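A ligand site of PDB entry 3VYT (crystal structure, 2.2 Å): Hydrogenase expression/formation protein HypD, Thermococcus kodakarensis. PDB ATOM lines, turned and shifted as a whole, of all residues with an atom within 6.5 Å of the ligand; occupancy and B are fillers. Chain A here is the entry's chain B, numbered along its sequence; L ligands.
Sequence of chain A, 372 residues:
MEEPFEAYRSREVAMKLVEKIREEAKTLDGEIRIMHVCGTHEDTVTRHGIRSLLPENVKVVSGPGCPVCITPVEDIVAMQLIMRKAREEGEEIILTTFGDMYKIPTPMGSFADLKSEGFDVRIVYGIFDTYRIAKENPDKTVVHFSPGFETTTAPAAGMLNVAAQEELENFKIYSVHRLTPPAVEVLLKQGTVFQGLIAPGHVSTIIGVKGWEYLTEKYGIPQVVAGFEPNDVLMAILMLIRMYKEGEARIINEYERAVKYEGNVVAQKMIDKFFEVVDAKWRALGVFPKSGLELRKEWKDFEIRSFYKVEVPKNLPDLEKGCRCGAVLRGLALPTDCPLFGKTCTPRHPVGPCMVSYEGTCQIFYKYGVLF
The side-chain sulfur (SG) of Cys 362 is bound to an iron atom (FE4) of the ligand, 2.2 Å away.
The side-chain sulfur (SG) of Cys 338 binds an iron atom (FE3) of the ligand, at 2.3 Å.
The side-chain sulfur (SG) of Cys 323 is bound to an iron atom (FE1) of the ligand (2.3 Å).
The side-chain sulfur (SG) of Cys 345 binds an iron atom (FE2) of the ligand, 2.3 Å away.
The backbone NH of Cys 325 sits close to a sulfur (S2) of the ligand.
N of Arg 324 lies close to S2 of the ligand (3.2 Å).
A sulfur (S3) of the ligand lies close to the backbone NH (N) of Met 355, 3.5 Å away.
N of Gly 352 lies close to S3 of the ligand, at 3.6 Å.
The backbone carbonyl oxygen (O) of Cys 354 is in hydrogen-bond range of the backbone NH (N) of Cys 362, 3.4 Å away.
The side-chain sulfur (SG) of Cys 338 sits close to the backbone NH (N) of Phe 341 (3.7 Å).
The backbone NH of Leu 340 sits close to the side-chain sulfur of Cys 338.
N of Cys 325 lies close to SG of Cys 323, at 3.5 Å.
O of Leu 340 lies within hydrogen-bond range of N of Cys 345, 3.1 Å away.
The side-chain sulfur (SG) of Cys 345 sits close to the backbone NH (N) of Val 351 (3.1 Å).
SG of Cys 354 is disulfide-bonded to SG of Cys 325, at 2.0 Å.
The backbone NH (N) of Gln 363 is in hydrogen-bond range of the backbone carbonyl oxygen (O) of Cys 354 (3.2 Å).
CB of Leu 340 touches S4 of the ligand (3.9 Å).
Phe 341 touches the ligand (CA to S1, 3.9 Å).
Val 351 touches the ligand.
Cys 354 touches the ligand.
Hydrophobic or aromatic side chains within 4 Å of the ligand: Leu 340, Phe 341, Val 351 and Met 355.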
ATOM      1  N   LEU A 319      20.693 -27.689   2.785  1.00  0.00           N
ATOM      2  CA  LEU A 319      20.816 -27.086   4.111  1.00  0.00           C
ATOM      3  C   LEU A 319      22.216 -26.548   4.330  1.00  0.00           C
ATOM      4  O   LEU A 319      23.137 -26.898   3.606  1.00  0.00           O
ATOM      5  CB  LEU A 319      20.542 -28.139   5.198  1.00  0.00           C
ATOM      6  CG  LEU A 319      19.212 -28.912   5.218  1.00  0.00           C
ATOM      7  CD1 LEU A 319      19.256 -30.001   6.281  1.00  0.00           C
ATOM      8  CD2 LEU A 319      18.075 -27.952   5.494  1.00  0.00           C
ATOM      9  N   GLY A 322      26.126 -28.356   9.157  1.00  0.00           N
ATOM     10  CA  GLY A 322      25.838 -28.439  10.581  1.00  0.00           C
ATOM     11  C   GLY A 322      24.371 -28.593  10.905  1.00  0.00           C
ATOM     12  O   GLY A 322      24.008 -29.118  11.959  1.00  0.00           O
ATOM     13  N   CYS A 323      23.512 -28.143   9.999  1.00  0.00           N
ATOM     14  CA  CYS A 323      22.071 -28.226  10.189  1.00  0.00           C
ATOM     15  C   CYS A 323      21.619 -29.680  10.059  1.00  0.00           C
ATOM     16  O   CYS A 323      22.042 -30.396   9.135  1.00  0.00           O
ATOM     17  CB  CYS A 323      21.366 -27.370   9.144  1.00  0.00           C
ATOM     18  SG  CYS A 323      19.549 -27.373   9.215  1.00  0.00           S
ATOM     19  N   ARG A 324      20.770 -30.117  10.984  1.00  0.00           N
ATOM     20  CA  ARG A 324      20.255 -31.486  10.990  1.00  0.00           C
ATOM     21  C   ARG A 324      18.738 -31.534  10.817  1.00  0.00           C
ATOM     22  O   ARG A 324      18.086 -32.503  11.228  1.00  0.00           O
ATOM     23  CB  ARG A 324      20.673 -32.164  12.290  1.00  0.00           C
ATOM     24  CG  ARG A 324      22.192 -32.250  12.379  1.00  0.00           C
ATOM     25  CD  ARG A 324      22.721 -32.170  13.790  1.00  0.00           C
ATOM     26  NE  ARG A 324      22.470 -33.381  14.552  1.00  0.00           N
ATOM     27  CZ  ARG A 324      23.376 -33.976  15.321  1.00  0.00           C
ATOM     28  NH1 ARG A 324      24.603 -33.464  15.406  1.00  0.00           N
ATOM     29  NH2 ARG A 324      23.067 -35.074  15.992  1.00  0.00           N
ATOM     30  N   CYS A 325      18.181 -30.499  10.191  1.00  0.00           N
ATOM     31  CA  CYS A 325      16.743 -30.388   9.960  1.00  0.00           C
ATOM     32  C   CYS A 325      16.209 -31.604   9.178  1.00  0.00           C
ATOM     33  O   CYS A 325      15.083 -32.049   9.399  1.00  0.00           O
ATOM     34  CB  CYS A 325      16.474 -29.063   9.239  1.00  0.00           C
ATOM     35  SG  CYS A 325      14.795 -28.705   8.631  1.00  0.00           S
ATOM     36  N   GLY A 326      17.041 -32.153   8.286  1.00  0.00           N
ATOM     37  CA  GLY A 326      16.654 -33.334   7.537  1.00  0.00           C
ATOM     38  C   GLY A 326      16.300 -34.483   8.472  1.00  0.00           C
ATOM     39  O   GLY A 326      15.291 -35.179   8.270  1.00  0.00           O
ATOM     40  N   VAL A 328      15.535 -34.100  11.679  1.00  0.00           N
ATOM     41  CA  VAL A 328      14.432 -33.611  12.512  1.00  0.00           C
ATOM     42  C   VAL A 328      13.123 -33.895  11.765  1.00  0.00           C
ATOM     43  O   VAL A 328      12.123 -34.351  12.340  1.00  0.00           O
ATOM     44  CB  VAL A 328      14.545 -32.088  12.743  1.00  0.00           C
ATOM     45  CG1 VAL A 328      13.236 -31.540  13.313  1.00  0.00           C
ATOM     46  CG2 VAL A 328      15.701 -31.784  13.694  1.00  0.00           C
ATOM     47  N   PRO A 335      15.703 -31.361  17.790  1.00  0.00           N
ATOM     48  CA  PRO A 335      16.425 -30.118  17.488  1.00  0.00           C
ATOM     49  C   PRO A 335      17.562 -29.828  18.472  1.00  0.00           C
ATOM     50  O   PRO A 335      18.572 -29.211  18.117  1.00  0.00           O
ATOM     51  CB  PRO A 335      15.317 -29.055  17.505  1.00  0.00           C
ATOM     52  CG  PRO A 335      14.258 -29.639  18.356  1.00  0.00           C
ATOM     53  CD  PRO A 335      14.257 -31.103  17.954  1.00  0.00           C
ATOM     54  N   CYS A 338      20.944 -30.919  17.690  1.00  0.00           N
ATOM     55  CA  CYS A 338      21.678 -30.066  16.781  1.00  0.00           C
ATOM     56  C   CYS A 338      22.637 -29.114  17.489  1.00  0.00           C
ATOM     57  O   CYS A 338      22.264 -28.428  18.433  1.00  0.00           O
ATOM     58  CB  CYS A 338      20.712 -29.275  15.940  1.00  0.00           C
ATOM     59  SG  CYS A 338      21.559 -28.170  14.795  1.00  0.00           S
ATOM     60  N   PRO A 339      23.884 -29.047  17.015  1.00  0.00           N
ATOM     61  CA  PRO A 339      24.889 -28.163  17.618  1.00  0.00           C
ATOM     62  C   PRO A 339      24.548 -26.679  17.489  1.00  0.00           C
ATOM     63  O   PRO A 339      24.923 -25.867  18.340  1.00  0.00           O
ATOM     64  CB  PRO A 339      26.169 -28.541  16.876  1.00  0.00           C
ATOM     65  CG  PRO A 339      25.657 -28.940  15.506  1.00  0.00           C
ATOM     66  CD  PRO A 339      24.448 -29.784  15.869  1.00  0.00           C
ATOM     67  N   LEU A 340      23.811 -26.338  16.446  1.00  0.00           N
ATOM     68  CA  LEU A 340      23.432 -24.949  16.192  1.00  0.00           C
ATOM     69  C   LEU A 340      22.179 -24.528  16.966  1.00  0.00           C
ATOM     70  O   LEU A 340      21.941 -23.337  17.182  1.00  0.00           O
ATOM     71  CB  LEU A 340      23.231 -24.750  14.694  1.00  0.00           C
ATOM     72  CG  LEU A 340      24.377 -25.342  13.872  1.00  0.00           C
ATOM     73  CD1 LEU A 340      24.186 -25.039  12.400  1.00  0.00           C
ATOM     74  CD2 LEU A 340      25.699 -24.771  14.356  1.00  0.00           C
ATOM     75  N   PHE A 341      21.376 -25.496  17.380  1.00  0.00           N
ATOM     76  CA  PHE A 341      20.160 -25.195  18.116  1.00  0.00           C
ATOM     77  C   PHE A 341      20.370 -24.218  19.263  1.00  0.00           C
ATOM     78  O   PHE A 341      21.114 -24.505  20.197  1.00  0.00           O
ATOM     79  CB  PHE A 341      19.536 -26.468  18.677  1.00  0.00           C
ATOM     80  CG  PHE A 341      18.205 -26.252  19.323  1.00  0.00           C
ATOM     81  CD1 PHE A 341      17.059 -26.126  18.557  1.00  0.00           C
ATOM     82  CD2 PHE A 341      18.099 -26.162  20.708  1.00  0.00           C
ATOM     83  CE1 PHE A 341      15.833 -25.934  19.157  1.00  0.00           C
ATOM     84  CE2 PHE A 341      16.874 -25.968  21.318  1.00  0.00           C
ATOM     85  CZ  PHE A 341      15.737 -25.844  20.541  1.00  0.00           C
ATOM     86  N   GLY A 342      19.675 -23.082  19.213  1.00  0.00           N
ATOM     87  CA  GLY A 342      19.769 -22.089  20.277  1.00  0.00           C
ATOM     88  C   GLY A 342      21.091 -21.366  20.336  1.00  0.00           C
ATOM     89  O   GLY A 342      21.309 -20.529  21.217  1.00  0.00           O
ATOM     90  N   CYS A 345      21.587 -20.648  15.607  1.00  0.00           N
ATOM     91  CA  CYS A 345      20.269 -20.827  15.029  1.00  0.00           C
ATOM     92  C   CYS A 345      19.138 -20.587  16.019  1.00  0.00           C
ATOM     93  O   CYS A 345      19.018 -21.288  17.025  1.00  0.00           O
ATOM     94  CB  CYS A 345      20.138 -22.237  14.440  1.00  0.00           C
ATOM     95  SG  CYS A 345      18.716 -22.443  13.328  1.00  0.00           S
ATOM     96  N   THR A 346      18.323 -19.578  15.724  1.00  0.00           N
ATOM     97  CA  THR A 346      17.169 -19.227  16.559  1.00  0.00           C
ATOM     98  C   THR A 346      16.130 -18.702  15.588  1.00  0.00           C
ATOM     99  O   THR A 346      16.427 -18.495  14.400  1.00  0.00           O
ATOM    100  CB  THR A 346      17.483 -18.110  17.607  1.00  0.00           C
ATOM    101  OG1 THR A 346      17.930 -16.931  16.933  1.00  0.00           O
ATOM    102  CG2 THR A 346      18.548 -18.575  18.587  1.00  0.00           C
ATOM    103  N   PRO A 350      17.671 -17.642  12.028  1.00  0.00           N
ATOM    104  CA  PRO A 350      17.666 -19.052  11.640  1.00  0.00           C
ATOM    105  C   PRO A 350      18.730 -19.490  10.652  1.00  0.00           C
ATOM    106  O   PRO A 350      19.070 -18.763   9.724  1.00  0.00           O
ATOM    107  CB  PRO A 350      16.256 -19.254  11.073  1.00  0.00           C
ATOM    108  CG  PRO A 350      15.974 -17.926  10.434  1.00  0.00           C
ATOM    109  CD  PRO A 350      16.497 -16.939  11.460  1.00  0.00           C
ATOM    110  N   VAL A 351      19.231 -20.691  10.859  1.00  0.00           N
ATOM    111  CA  VAL A 351      20.223 -21.260   9.976  1.00  0.00           C
ATOM    112  C   VAL A 351      19.517 -22.231   9.045  1.00  0.00           C
ATOM    113  O   VAL A 351      19.801 -22.287   7.852  1.00  0.00           O
ATOM    114  CB  VAL A 351      21.299 -22.006  10.761  1.00  0.00           C
ATOM    115  CG1 VAL A 351      22.334 -22.572   9.782  1.00  0.00           C
ATOM    116  CG2 VAL A 351      21.978 -21.054  11.758  1.00  0.00           C
ATOM    117  N   GLY A 352      18.571 -22.988   9.595  1.00  0.00           N
ATOM    118  CA  GLY A 352      17.836 -23.975   8.821  1.00  0.00           C
ATOM    119  C   GLY A 352      16.369 -23.662   8.646  1.00  0.00           C
ATOM    120  O   GLY A 352      15.840 -22.797   9.347  1.00  0.00           O
ATOM    121  N   PRO A 353      15.657 -24.375   7.751  1.00  0.00           N
ATOM    122  CA  PRO A 353      14.227 -24.086   7.566  1.00  0.00           C
ATOM    123  C   PRO A 353      13.346 -24.518   8.726  1.00  0.00           C
ATOM    124  O   PRO A 353      12.334 -23.879   9.014  1.00  0.00           O
ATOM    125  CB  PRO A 353      13.904 -24.804   6.253  1.00  0.00           C
ATOM    126  CG  PRO A 353      14.885 -25.942   6.217  1.00  0.00           C
ATOM    127  CD  PRO A 353      16.154 -25.349   6.764  1.00  0.00           C
ATOM    128  N   CYS A 354      13.733 -25.585   9.401  1.00  0.00           N
ATOM    129  CA  CYS A 354      12.977 -26.087  10.559  1.00  0.00           C
ATOM    130  C   CYS A 354      12.828 -25.039  11.677  1.00  0.00           C
ATOM    131  O   CYS A 354      11.887 -25.105  12.459  1.00  0.00           O
ATOM    132  CB  CYS A 354      13.654 -27.331  11.131  1.00  0.00           C
ATOM    133  SG  CYS A 354      13.533 -28.908  10.219  1.00  0.00           S
ATOM    134  N   MET A 355      13.758 -24.091  11.761  1.00  0.00           N
ATOM    135  CA  MET A 355      13.712 -23.062  12.792  1.00  0.00           C
ATOM    136  C   MET A 355      12.890 -21.844  12.327  1.00  0.00           C
ATOM    137  O   MET A 355      12.242 -21.180  13.126  1.00  0.00           O
ATOM    138  CB  MET A 355      15.145 -22.627  13.164  1.00  0.00           C
ATOM    139  CG  MET A 355      15.248 -21.603  14.304  1.00  0.00           C
ATOM    140  SD  MET A 355      14.596 -22.206  15.881  1.00  0.00           S
ATOM    141  CE  MET A 355      15.985 -23.142  16.480  1.00  0.00           C
ATOM    142  N   VAL A 356      12.921 -21.584  11.024  1.00  0.00           N
ATOM    143  CA  VAL A 356      12.200 -20.473  10.422  1.00  0.00           C
ATOM    144  C   VAL A 356      10.684 -20.652  10.399  1.00  0.00           C
ATOM    145  O   VAL A 356       9.920 -19.731  10.728  1.00  0.00           O
ATOM    146  CB  VAL A 356      12.607 -20.253   8.949  1.00  0.00           C
ATOM    147  CG1 VAL A 356      11.833 -19.084   8.375  1.00  0.00           C
ATOM    148  CG2 VAL A 356      14.088 -20.019   8.847  1.00  0.00           C
ATOM    149  N   THR A 361       9.674 -27.894  13.607  1.00  0.00           N
ATOM    150  CA  THR A 361       9.880 -28.549  14.882  1.00  0.00           C
ATOM    151  C   THR A 361      10.922 -27.817  15.724  1.00  0.00           C
ATOM    152  O   THR A 361      10.764 -27.706  16.939  1.00  0.00           O
ATOM    153  CB  THR A 361      10.289 -29.994  14.674  1.00  0.00           C
ATOM    154  OG1 THR A 361       9.259 -30.664  13.924  1.00  0.00           O
ATOM    155  CG2 THR A 361      10.465 -30.719  16.022  1.00  0.00           C
ATOM    156  N   CYS A 362      11.971 -27.313  15.087  1.00  0.00           N
ATOM    157  CA  CYS A 362      13.004 -26.576  15.818  1.00  0.00           C
ATOM    158  C   CYS A 362      12.482 -25.272  16.399  1.00  0.00           C
ATOM    159  O   CYS A 362      12.793 -24.911  17.548  1.00  0.00           O
ATOM    160  CB  CYS A 362      14.195 -26.283  14.903  1.00  0.00           C
ATOM    161  SG  CYS A 362      15.091 -27.798  14.449  1.00  0.00           S
ATOM    162  N   GLN A 363      11.676 -24.554  15.625  1.00  0.00           N
ATOM    163  CA  GLN A 363      11.132 -23.304  16.103  1.00  0.00           C
ATOM    164  C   GLN A 363      10.214 -23.580  17.275  1.00  0.00           C
ATOM    165  O   GLN A 363      10.211 -22.843  18.270  1.00  0.00           O
ATOM    166  CB  GLN A 363      10.341 -22.582  15.003  1.00  0.00           C
ATOM    167  CG  GLN A 363       9.985 -21.165  15.402  1.00  0.00           C
ATOM    168  CD  GLN A 363       9.229 -20.410  14.335  1.00  0.00           C
ATOM    169  OE1 GLN A 363       8.003 -20.384  14.329  1.00  0.00           O
ATOM    170  NE2 GLN A 363       9.964 -19.792  13.417  1.00  0.00           N
HETATM  171 FE1  LIG L   1      18.645 -26.840  11.250  1.00  0.00          FE
HETATM  172 FE2  LIG L   1      18.571 -24.764  13.024  1.00  0.00          FE
HETATM  173 FE3  LIG L   1      19.703 -27.226  13.871  1.00  0.00          FE
HETATM  174 FE4  LIG L   1      16.972 -27.113  13.572  1.00  0.00          FE
HETATM  175  S1  LIG L   1      18.227 -25.744  14.807  1.00  0.00           S
HETATM  176  S2  LIG L   1      18.419 -28.465  12.399  1.00  0.00           S
HETATM  177  S3  LIG L   1      16.989 -25.324  11.903  1.00  0.00           S
HETATM  178  S4  LIG L   1      20.236 -25.500  12.306  1.00  0.00           S
